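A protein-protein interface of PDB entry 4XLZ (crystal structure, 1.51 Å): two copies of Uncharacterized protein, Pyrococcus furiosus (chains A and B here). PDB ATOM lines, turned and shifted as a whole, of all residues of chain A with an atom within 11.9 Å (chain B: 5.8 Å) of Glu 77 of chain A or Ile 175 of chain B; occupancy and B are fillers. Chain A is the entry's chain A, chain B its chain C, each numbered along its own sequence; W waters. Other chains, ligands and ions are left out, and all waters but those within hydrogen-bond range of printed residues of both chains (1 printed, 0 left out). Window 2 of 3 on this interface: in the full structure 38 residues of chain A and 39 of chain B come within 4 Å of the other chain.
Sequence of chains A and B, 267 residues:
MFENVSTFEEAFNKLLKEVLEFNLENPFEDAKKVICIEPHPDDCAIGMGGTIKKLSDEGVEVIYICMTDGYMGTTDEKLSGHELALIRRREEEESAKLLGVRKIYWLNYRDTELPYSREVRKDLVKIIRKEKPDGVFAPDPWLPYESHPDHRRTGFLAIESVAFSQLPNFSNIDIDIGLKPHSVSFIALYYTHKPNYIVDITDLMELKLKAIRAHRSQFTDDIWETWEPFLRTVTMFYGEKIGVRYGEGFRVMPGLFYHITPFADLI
The backbone NH (N) of Phe 170 of chain B sits at hydrogen-bond distance from the side-chain sulfur (SD) of Met 72 of chain A (3.6 Å). OE1 of Glu 77 of chain A lies within salt-bridge range of NZ of Lys 180 of chain B (3.9 Å).
The side-chain hydroxyl of Thr 74 of chain A lies within hydrogen-bond range of the backbone NH of Asp 76 of chain A (2.9 Å). OD2 of Asp 76 of chain A lies within salt-bridge range of NZ of Lys 78 of chain A (3.0 Å). The backbone carbonyl oxygen (O) of Leu 167 of chain B is in hydrogen-bond range of the guanidinium group (NH1) of Arg 129 of chain B (2.9 Å). The guanidinium group (NH1) of Arg 129 of chain B is in hydrogen-bond range of the backbone carbonyl oxygen (O) of Phe 170 of chain B (2.9 Å).
Leu 167 of chain B touches Met 72 of chain A. Thr 74 of chain A touches Leu 167 of chain B (O to CD2, 3.8 Å). Thr 74 of chain A touches Pro 168 of chain B (O to CD, 3.4 Å). CD of Pro 168 of chain B touches CA of Thr 75 of chain A, 3.6 Å away. Pro 168 of chain B touches Asp 76 of chain A. CB of Pro 168 of chain B touches CG of Glu 77 of chain A, at 3.6 Å. Ile 175 of chain B touches Glu 77 of chain A. CD of Pro 181 of chain B touches OE1 of Glu 77 of chain A (3.7 Å).
Printed residues of chain B within 4 Å of Met 72 of chain A: Leu 167 and Phe 170. Of the printed residues of chain B, Thr 74 of chain A touches Leu 167 and Pro 168. Printed residues of chain B within 4 Å of Thr 75 of chain A: Pro 168. Printed residues of chain B within 4 Å of Asp 76 of chain A: Pro 168. Of chain B, only Pro 168 (3.6 Å), Ile 175 (3.6 Å), Lys 180 (3.9 Å) and Pro 181 (3.7 Å) come within 4 Å of Glu 77 of chain A. Gly 81 of chain A touches none of the printed residues of chain B. Of the printed residues of chain A, Leu 167 of chain B touches Met 72 (3.8 Å) and Thr 74 (3.8 Å). Pro 168 of chain B touches just these residues of chain A: Thr 74 (3.4 Å), Thr 75 (3.6 Å), Asp 76 (3.8 Å) and Glu 77 (3.6 Å). Ser 171 of chain B touches none of the printed residues of chain A. No residue of chain A comes within 4 Å of Asn 172 of chain B. No residue of chain A comes within 4 Å of Ile 173 of chain B. No residue of chain A comes within 4 Å of Asp 174 of chain B. Ile 175 of chain B touches one residue of chain A. No residue of chain A comes within 4 Å of Asp 176 of chain B. No residue of chain A comes within 4 Å of Ile 177 of chain B. No residue of chain A comes within 4 Å of Gly 178 of chain B. No residue of chain A comes within 4 Å of Leu 179 of chain B. Printed residues of chain A within 4 Å of Lys 180 of chain B: Glu 77.
Of the 15 printed residues of chain B, 6 touch a printed residue of chain A.
No position is printed for both chains.
Water W1 bridges the side-chain hydroxyl of Tyr 71 of chain A and the side-chain amide oxygen of Asn 172 of chain B.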
ATOM      1  N   TYR A  71      -3.294  -9.499   5.562  1.00  0.00           N
ATOM      2  CA  TYR A  71      -2.606  -8.299   5.045  1.00  0.00           C
ATOM      3  C   TYR A  71      -1.151  -8.496   4.725  1.00  0.00           C
ATOM      4  O   TYR A  71      -0.598  -7.809   3.870  1.00  0.00           O
ATOM      5  CB  TYR A  71      -2.831  -7.187   6.155  1.00  0.00           C
ATOM      6  CG  TYR A  71      -2.255  -5.848   5.924  1.00  0.00           C
ATOM      7  CD1 TYR A  71      -3.130  -4.784   5.554  1.00  0.00           C
ATOM      8  CD2 TYR A  71      -0.912  -5.577   6.178  1.00  0.00           C
ATOM      9  CE1 TYR A  71      -2.644  -3.471   5.441  1.00  0.00           C
ATOM     10  CE2 TYR A  71      -0.392  -4.298   6.061  1.00  0.00           C
ATOM     11  CZ  TYR A  71      -1.295  -3.245   5.710  1.00  0.00           C
ATOM     12  OH  TYR A  71      -0.784  -1.976   5.585  1.00  0.00           O
ATOM     13  N   MET A  72      -0.473  -9.321   5.544  1.00  0.00           N
ATOM     14  CA  MET A  72       0.985  -9.347   5.458  1.00  0.00           C
ATOM     15  C   MET A  72       1.485 -10.412   4.487  1.00  0.00           C
ATOM     16  O   MET A  72       2.723 -10.497   4.263  1.00  0.00           O
ATOM     17  CB  MET A  72       1.601  -9.676   6.836  1.00  0.00           C
ATOM     18  CG  MET A  72       1.342  -8.570   7.822  1.00  0.00           C
ATOM     19  SD  MET A  72       2.416  -6.976   7.356  1.00  0.00           S
ATOM     20  CE  MET A  72       1.667  -5.927   8.823  1.00  0.00           C
ATOM     21  N   GLY A  73       0.584 -11.246   3.962  1.00  0.00           N
ATOM     22  CA  GLY A  73       1.024 -12.427   3.166  1.00  0.00           C
ATOM     23  C   GLY A  73       1.583 -12.177   1.768  1.00  0.00           C
ATOM     24  O   GLY A  73       1.025 -12.793   0.793  1.00  0.00           O
ATOM     25  N   THR A  74       2.497 -11.264   1.579  1.00  0.00           N
ATOM     26  CA  THR A  74       3.077 -11.110   0.215  1.00  0.00           C
ATOM     27  C   THR A  74       4.545 -10.686   0.351  1.00  0.00           C
ATOM     28  O   THR A  74       4.934 -10.018   1.273  1.00  0.00           O
ATOM     29  CB  THR A  74       2.287 -10.027  -0.624  1.00  0.00           C
ATOM     30  OG1 THR A  74       2.929  -9.831  -1.952  1.00  0.00           O
ATOM     31  CG2 THR A  74       2.292  -8.617   0.015  1.00  0.00           C
ATOM     32  N   THR A  75       5.406 -11.057  -0.648  1.00  0.00           N
ATOM     33  CA  THR A  75       6.749 -10.481  -0.727  1.00  0.00           C
ATOM     34  C   THR A  75       6.872  -9.582  -1.943  1.00  0.00           C
ATOM     35  O   THR A  75       7.935  -9.044  -2.188  1.00  0.00           O
ATOM     36  CB  THR A  75       7.839 -11.587  -0.795  1.00  0.00           C
ATOM     37  OG1 THR A  75       7.561 -12.399  -1.950  1.00  0.00           O
ATOM     38  CG2 THR A  75       7.795 -12.500   0.399  1.00  0.00           C
ATOM     39  N   ASP A  76       5.725  -9.272  -2.600  1.00  0.00           N
ATOM     40  CA  ASP A  76       5.727  -8.224  -3.675  1.00  0.00           C
ATOM     41  C   ASP A  76       5.710  -6.804  -3.107  1.00  0.00           C
ATOM     42  O   ASP A  76       4.659  -6.341  -2.471  1.00  0.00           O
ATOM     43  CB  ASP A  76       4.527  -8.517  -4.588  1.00  0.00           C
ATOM     44  CG  ASP A  76       4.410  -7.497  -5.770  1.00  0.00           C
ATOM     45  OD1 ASP A  76       3.494  -7.678  -6.552  1.00  0.00           O
ATOM     46  OD2 ASP A  76       5.174  -6.505  -5.826  1.00  0.00           O
ATOM     47  N   GLU A  77       6.801  -6.014  -3.285  1.00  0.00           N
ATOM     48  CA  GLU A  77       6.876  -4.616  -2.788  1.00  0.00           C
ATOM     49  C   GLU A  77       5.796  -3.703  -3.469  1.00  0.00           C
ATOM     50  O   GLU A  77       5.476  -2.619  -2.921  1.00  0.00           O
ATOM     51  CB  GLU A  77       8.258  -3.939  -2.995  1.00  0.00           C
ATOM     52  CG  GLU A  77       9.311  -4.178  -1.846  1.00  0.00           C
ATOM     53  CD  GLU A  77      10.656  -3.500  -2.134  1.00  0.00           C
ATOM     54  OE1 GLU A  77      11.636  -4.259  -2.324  1.00  0.00           O
ATOM     55  OE2 GLU A  77      10.694  -2.242  -2.270  1.00  0.00           O
ATOM     56  N   LYS A  78       5.215  -4.162  -4.587  1.00  0.00           N
ATOM     57  CA  LYS A  78       4.162  -3.284  -5.191  1.00  0.00           C
ATOM     58  C   LYS A  78       2.744  -3.637  -4.699  1.00  0.00           C
ATOM     59  O   LYS A  78       1.756  -2.975  -5.156  1.00  0.00           O
ATOM     60  CB  LYS A  78       4.215  -3.331  -6.741  1.00  0.00           C
ATOM     61  CG  LYS A  78       5.493  -2.528  -7.302  1.00  0.00           C
ATOM     62  CD  LYS A  78       5.822  -2.937  -8.810  1.00  0.00           C
ATOM     63  CE  LYS A  78       5.363  -4.414  -9.187  1.00  0.00           C
ATOM     64  NZ  LYS A  78       6.127  -5.576  -8.531  1.00  0.00           N
ATOM     65  N   LEU A  79       2.569  -4.672  -3.890  1.00  0.00           N
ATOM     66  CA  LEU A  79       1.179  -5.053  -3.542  1.00  0.00           C
ATOM     67  C   LEU A  79       0.926  -4.588  -2.091  1.00  0.00           C
ATOM     68  O   LEU A  79       1.565  -5.198  -1.180  1.00  0.00           O
ATOM     69  CB  LEU A  79       1.070  -6.519  -3.601  1.00  0.00           C
ATOM     70  CG  LEU A  79      -0.290  -7.099  -3.267  1.00  0.00           C
ATOM     71  CD1 LEU A  79      -1.376  -6.474  -4.203  1.00  0.00           C
ATOM     72  CD2 LEU A  79      -0.346  -8.624  -3.328  1.00  0.00           C
ATOM     73  N   SER A  80       0.006  -3.659  -1.930  1.00  0.00           N
ATOM     74  CA  SER A  80      -0.239  -3.136  -0.542  1.00  0.00           C
ATOM     75  C   SER A  80      -0.961  -4.264   0.190  1.00  0.00           C
ATOM     76  O   SER A  80      -1.663  -5.137  -0.344  1.00  0.00           O
ATOM     77  CB  SER A  80      -1.096  -1.873  -0.606  1.00  0.00           C
ATOM     78  OG  SER A  80      -2.436  -2.155  -1.003  1.00  0.00           O
ATOM     79  N   GLY A  81      -0.918  -4.136   1.542  1.00  0.00           N
ATOM     80  CA  GLY A  81      -1.703  -5.098   2.329  1.00  0.00           C
ATOM     81  C   GLY A  81      -3.217  -4.982   2.202  1.00  0.00           C
ATOM     82  O   GLY A  81      -3.951  -5.915   2.345  1.00  0.00           O
ATOM     83  N   HIS A  82      -3.623  -3.743   1.921  1.00  0.00           N
ATOM     84  CA  HIS A  82      -5.049  -3.501   1.694  1.00  0.00           C
ATOM     85  C   HIS A  82      -5.577  -4.266   0.447  1.00  0.00           C
ATOM     86  O   HIS A  82      -6.617  -4.957   0.500  1.00  0.00           O
ATOM     87  CB  HIS A  82      -5.342  -2.019   1.493  1.00  0.00           C
ATOM     88  CG  HIS A  82      -4.821  -1.153   2.579  1.00  0.00           C
ATOM     89  ND1 HIS A  82      -5.253  -1.316   3.884  1.00  0.00           N
ATOM     90  CD2 HIS A  82      -3.963  -0.119   2.585  1.00  0.00           C
ATOM     91  CE1 HIS A  82      -4.647  -0.430   4.628  1.00  0.00           C
ATOM     92  NE2 HIS A  82      -3.864   0.320   3.902  1.00  0.00           N
ATOM     93  N   GLU A  83      -4.783  -4.076  -0.626  1.00  0.00           N
ATOM     94  CA  GLU A  83      -5.118  -4.850  -1.812  1.00  0.00           C
ATOM     95  C   GLU A  83      -5.057  -6.352  -1.637  1.00  0.00           C
ATOM     96  O   GLU A  83      -5.959  -7.099  -2.024  1.00  0.00           O
ATOM     97  CB  GLU A  83      -4.324  -4.404  -3.040  1.00  0.00           C
ATOM     98  CG  GLU A  83      -4.894  -5.049  -4.345  1.00  0.00           C
ATOM     99  CD  GLU A  83      -4.259  -4.428  -5.632  1.00  0.00           C
ATOM    100  OE1 GLU A  83      -3.374  -3.535  -5.535  1.00  0.00           O
ATOM    101  OE2 GLU A  83      -4.764  -4.912  -6.737  1.00  0.00           O
ATOM    102  N   LEU A  84      -4.002  -6.838  -0.919  1.00  0.00           N
ATOM    103  CA  LEU A  84      -3.893  -8.259  -0.610  1.00  0.00           C
ATOM    104  C   LEU A  84      -5.106  -8.742   0.137  1.00  0.00           C
ATOM    105  O   LEU A  84      -5.660  -9.793  -0.064  1.00  0.00           O
ATOM    106  CB  LEU A  84      -2.591  -8.528   0.100  1.00  0.00           C
ATOM    107  CG  LEU A  84      -2.463  -9.949   0.445  1.00  0.00           C
ATOM    108  CD1 LEU A  84      -2.389 -10.900  -0.866  1.00  0.00           C
ATOM    109  CD2 LEU A  84      -1.066 -10.107   1.144  1.00  0.00           C
ATOM    110  N   ILE A  87      -7.994  -9.191  -2.072  1.00  0.00           N
ATOM    111  CA  ILE A  87      -7.799 -10.381  -2.930  1.00  0.00           C
ATOM    112  C   ILE A  87      -8.031 -11.659  -2.142  1.00  0.00           C
ATOM    113  O   ILE A  87      -8.713 -12.642  -2.568  1.00  0.00           O
ATOM    114  CB  ILE A  87      -6.372 -10.384  -3.483  1.00  0.00           C
ATOM    115  CG1 ILE A  87      -6.214  -9.285  -4.564  1.00  0.00           C
ATOM    116  CG2 ILE A  87      -5.931 -11.798  -4.000  1.00  0.00           C
ATOM    117  CD1 ILE A  87      -4.749  -8.952  -4.854  1.00  0.00           C
ATOM    118  N   SER A 217      -2.847 -16.108  -4.230  1.00  0.00           N
ATOM    119  CA  SER A 217      -1.842 -15.147  -3.826  1.00  0.00           C
ATOM    120  C   SER A 217      -0.812 -15.751  -2.862  1.00  0.00           C
ATOM    121  O   SER A 217       0.324 -15.214  -2.744  1.00  0.00           O
ATOM    122  CB  SER A 217      -2.591 -13.971  -3.064  1.00  0.00           C
ATOM    123  OG  SER A 217      -3.179 -14.474  -1.885  1.00  0.00           O
ATOM    124  N   ARG B 129      17.235  -5.672   8.563  1.00  0.00           N
ATOM    125  CA  ARG B 129      17.244  -5.150   7.155  1.00  0.00           C
ATOM    126  C   ARG B 129      18.464  -4.274   6.983  1.00  0.00           C
ATOM    127  O   ARG B 129      18.987  -4.287   5.785  1.00  0.00           O
ATOM    128  CB  ARG B 129      15.952  -4.322   6.914  1.00  0.00           C
ATOM    129  CG  ARG B 129      14.803  -5.265   6.848  1.00  0.00           C
ATOM    130  CD  ARG B 129      13.489  -4.349   6.783  1.00  0.00           C
ATOM    131  NE  ARG B 129      12.329  -5.237   6.538  1.00  0.00           N
ATOM    132  CZ  ARG B 129      11.030  -4.833   6.654  1.00  0.00           C
ATOM    133  NH1 ARG B 129      10.057  -5.669   6.338  1.00  0.00           N
ATOM    134  NH2 ARG B 129      10.774  -3.618   7.174  1.00  0.00           N
ATOM    135  N   LEU B 167       9.039  -9.332   4.679  1.00  0.00           N
ATOM    136  CA  LEU B 167       7.675  -8.922   4.209  1.00  0.00           C
ATOM    137  C   LEU B 167       7.607  -7.460   4.069  1.00  0.00           C
ATOM    138  O   LEU B 167       7.719  -6.637   5.003  1.00  0.00           O
ATOM    139  CB  LEU B 167       6.610  -9.308   5.325  1.00  0.00           C
ATOM    140  CG  LEU B 167       6.577 -10.782   5.658  1.00  0.00           C
ATOM    141  CD1 LEU B 167       5.553 -11.111   6.747  1.00  0.00           C
ATOM    142  CD2 LEU B 167       6.309 -11.680   4.425  1.00  0.00           C
ATOM    143  N   PRO B 168       7.466  -6.888   2.816  1.00  0.00           N
ATOM    144  CA  PRO B 168       7.554  -5.451   2.612  1.00  0.00           C
ATOM    145  C   PRO B 168       6.381  -4.574   3.265  1.00  0.00           C
ATOM    146  O   PRO B 168       6.577  -3.400   3.494  1.00  0.00           O
ATOM    147  CB  PRO B 168       7.499  -5.299   1.051  1.00  0.00           C
ATOM    148  CG  PRO B 168       6.908  -6.530   0.609  1.00  0.00           C
ATOM    149  CD  PRO B 168       7.327  -7.686   1.540  1.00  0.00           C
ATOM    150  N   PHE B 170       5.421  -5.292   6.237  1.00  0.00           N
ATOM    151  CA  PHE B 170       5.687  -5.240   7.704  1.00  0.00           C
ATOM    152  C   PHE B 170       6.681  -4.100   7.904  1.00  0.00           C
ATOM    153  O   PHE B 170       7.797  -4.063   7.321  1.00  0.00           O
ATOM    154  CB  PHE B 170       6.301  -6.612   8.170  1.00  0.00           C
ATOM    155  CG  PHE B 170       6.519  -6.630   9.676  1.00  0.00           C
ATOM    156  CD1 PHE B 170       5.461  -7.199  10.445  1.00  0.00           C
ATOM    157  CD2 PHE B 170       7.630  -6.042  10.301  1.00  0.00           C
ATOM    158  CE1 PHE B 170       5.572  -7.237  11.848  1.00  0.00           C
ATOM    159  CE2 PHE B 170       7.691  -6.013  11.754  1.00  0.00           C
ATOM    160  CZ  PHE B 170       6.658  -6.583  12.406  1.00  0.00           C
ATOM    161  N   SER B 171       6.343  -3.192   8.855  1.00  0.00           N
ATOM    162  CA  SER B 171       7.216  -2.042   9.057  1.00  0.00           C
ATOM    163  C   SER B 171       7.612  -1.357   7.735  1.00  0.00           C
ATOM    164  O   SER B 171       8.795  -1.183   7.388  1.00  0.00           O
ATOM    165  CB  SER B 171       8.378  -2.400   9.978  1.00  0.00           C
ATOM    166  OG  SER B 171       8.900  -1.260  10.601  1.00  0.00           O
ATOM    167  N   ASN B 172       6.544  -0.887   7.024  1.00  0.00           N
ATOM    168  CA  ASN B 172       6.738  -0.473   5.642  1.00  0.00           C
ATOM    169  C   ASN B 172       7.536   0.807   5.589  1.00  0.00           C
ATOM    170  O   ASN B 172       8.105   1.082   4.485  1.00  0.00           O
ATOM    171  CB  ASN B 172       5.367  -0.319   4.921  1.00  0.00           C
ATOM    172  CG  ASN B 172       4.501   0.828   5.494  1.00  0.00           C
ATOM    173  OD1 ASN B 172       4.108   0.759   6.611  1.00  0.00           O
ATOM    174  ND2 ASN B 172       4.490   1.947   4.843  1.00  0.00           N
ATOM    175  N   ILE B 173       7.698   1.639   6.617  1.00  0.00           N
ATOM    176  CA  ILE B 173       8.434   2.891   6.462  1.00  0.00           C
ATOM    177  C   ILE B 173       9.958   2.524   6.284  1.00  0.00           C
ATOM    178  O   ILE B 173      10.671   3.270   5.657  1.00  0.00           O
ATOM    179  CB  ILE B 173       8.250   3.810   7.667  1.00  0.00           C
ATOM    180  CG1 ILE B 173       6.788   4.133   7.866  1.00  0.00           C
ATOM    181  CG2 ILE B 173       9.041   5.156   7.537  1.00  0.00           C
ATOM    182  CD1 ILE B 173       6.036   4.680   6.550  1.00  0.00           C
ATOM    183  N   ASP B 174      10.441   1.365   6.748  1.00  0.00           N
ATOM    184  CA  ASP B 174      11.841   0.935   6.456  1.00  0.00           C
ATOM    185  C   ASP B 174      11.991   0.920   4.925  1.00  0.00           C
ATOM    186  O   ASP B 174      13.013   1.428   4.498  1.00  0.00           O
ATOM    187  CB  ASP B 174      11.973  -0.541   6.961  1.00  0.00           C
ATOM    188  CG  ASP B 174      12.199  -0.627   8.426  1.00  0.00           C
ATOM    189  OD1 ASP B 174      12.290  -1.809   8.889  1.00  0.00           O
ATOM    190  OD2 ASP B 174      12.442   0.425   9.095  1.00  0.00           O
ATOM    191  N   ILE B 175      11.084   0.289   4.217  1.00  0.00           N
ATOM    192  CA  ILE B 175      11.214   0.136   2.742  1.00  0.00           C
ATOM    193  C   ILE B 175      11.208   1.540   2.160  1.00  0.00           C
ATOM    194  O   ILE B 175      12.035   1.878   1.300  1.00  0.00           O
ATOM    195  CB  ILE B 175      10.054  -0.652   2.234  1.00  0.00           C
ATOM    196  CG1 ILE B 175      10.251  -2.183   2.352  1.00  0.00           C
ATOM    197  CG2 ILE B 175       9.821  -0.438   0.731  1.00  0.00           C
ATOM    198  CD1 ILE B 175      10.625  -2.780   3.695  1.00  0.00           C
ATOM    199  N   ASP B 176      10.344   2.433   2.705  1.00  0.00           N
ATOM    200  CA  ASP B 176      10.253   3.779   2.141  1.00  0.00           C
ATOM    201  C   ASP B 176      11.489   4.587   2.332  1.00  0.00           C
ATOM    202  O   ASP B 176      11.695   5.542   1.582  1.00  0.00           O
ATOM    203  CB  ASP B 176       9.088   4.612   2.776  1.00  0.00           C
ATOM    204  CG  ASP B 176       7.736   3.932   2.542  1.00  0.00           C
ATOM    205  OD1 ASP B 176       6.813   4.090   3.355  1.00  0.00           O
ATOM    206  OD2 ASP B 176       7.602   3.139   1.560  1.00  0.00           O
ATOM    207  N   ILE B 177      12.318   4.333   3.367  1.00  0.00           N
ATOM    208  CA  ILE B 177      13.595   5.043   3.608  1.00  0.00           C
ATOM    209  C   ILE B 177      14.758   4.285   3.103  1.00  0.00           C
ATOM    210  O   ILE B 177      15.883   4.781   3.334  1.00  0.00           O
ATOM    211  CB  ILE B 177      13.825   5.441   5.035  1.00  0.00           C
ATOM    212  CG1 ILE B 177      14.015   4.222   5.998  1.00  0.00           C
ATOM    213  CG2 ILE B 177      12.644   6.349   5.603  1.00  0.00           C
ATOM    214  CD1 ILE B 177      14.674   4.599   7.338  1.00  0.00           C
ATOM    215  N   GLY B 178      14.549   3.197   2.373  1.00  0.00           N
ATOM    216  CA  GLY B 178      15.653   2.542   1.641  1.00  0.00           C
ATOM    217  C   GLY B 178      16.190   1.292   2.314  1.00  0.00           C
ATOM    218  O   GLY B 178      17.171   0.662   1.828  1.00  0.00           O
ATOM    219  N   LEU B 179      15.568   0.856   3.412  1.00  0.00           N
ATOM    220  CA  LEU B 179      15.889  -0.468   4.001  1.00  0.00           C
ATOM    221  C   LEU B 179      15.039  -1.592   3.453  1.00  0.00           C
ATOM    222  O   LEU B 179      13.831  -1.774   3.960  1.00  0.00           O
ATOM    223  CB  LEU B 179      15.703  -0.508   5.569  1.00  0.00           C
ATOM    224  CG  LEU B 179      16.541   0.466   6.287  1.00  0.00           C
ATOM    225  CD1 LEU B 179      16.019   0.486   7.743  1.00  0.00           C
ATOM    226  CD2 LEU B 179      18.005  -0.022   6.304  1.00  0.00           C
ATOM    227  N   LYS B 180      15.587  -2.365   2.508  1.00  0.00           N
ATOM    228  CA  LYS B 180      14.776  -3.278   1.769  1.00  0.00           C
ATOM    229  C   LYS B 180      14.499  -4.573   2.594  1.00  0.00           C
ATOM    230  O   LYS B 180      15.241  -4.866   3.592  1.00  0.00           O
ATOM    231  CB  LYS B 180      15.615  -3.691   0.552  1.00  0.00           C
ATOM    232  CG  LYS B 180      15.389  -2.593  -0.575  1.00  0.00           C
ATOM    233  CD  LYS B 180      16.344  -2.852  -1.761  1.00  0.00           C
ATOM    234  CE  LYS B 180      16.077  -1.865  -2.950  1.00  0.00           C
ATOM    235  NZ  LYS B 180      14.591  -1.896  -3.351  1.00  0.00           N
ATOM    236  N   PRO B 181      13.549  -5.378   2.206  1.00  0.00           N
ATOM    237  CA  PRO B 181      13.279  -6.678   2.868  1.00  0.00           C
ATOM    238  C   PRO B 181      14.584  -7.487   2.845  1.00  0.00           C
ATOM    239  O   PRO B 181      15.424  -7.355   1.863  1.00  0.00           O
ATOM    240  CB  PRO B 181      12.235  -7.340   2.031  1.00  0.00           C
ATOM    241  CG  PRO B 181      11.450  -6.118   1.401  1.00  0.00           C
ATOM    242  CD  PRO B 181      12.528  -5.107   1.130  1.00  0.00           C
HETATM  243  O   HOH W   1       1.867  -1.653   5.920  1.00  0.00           O
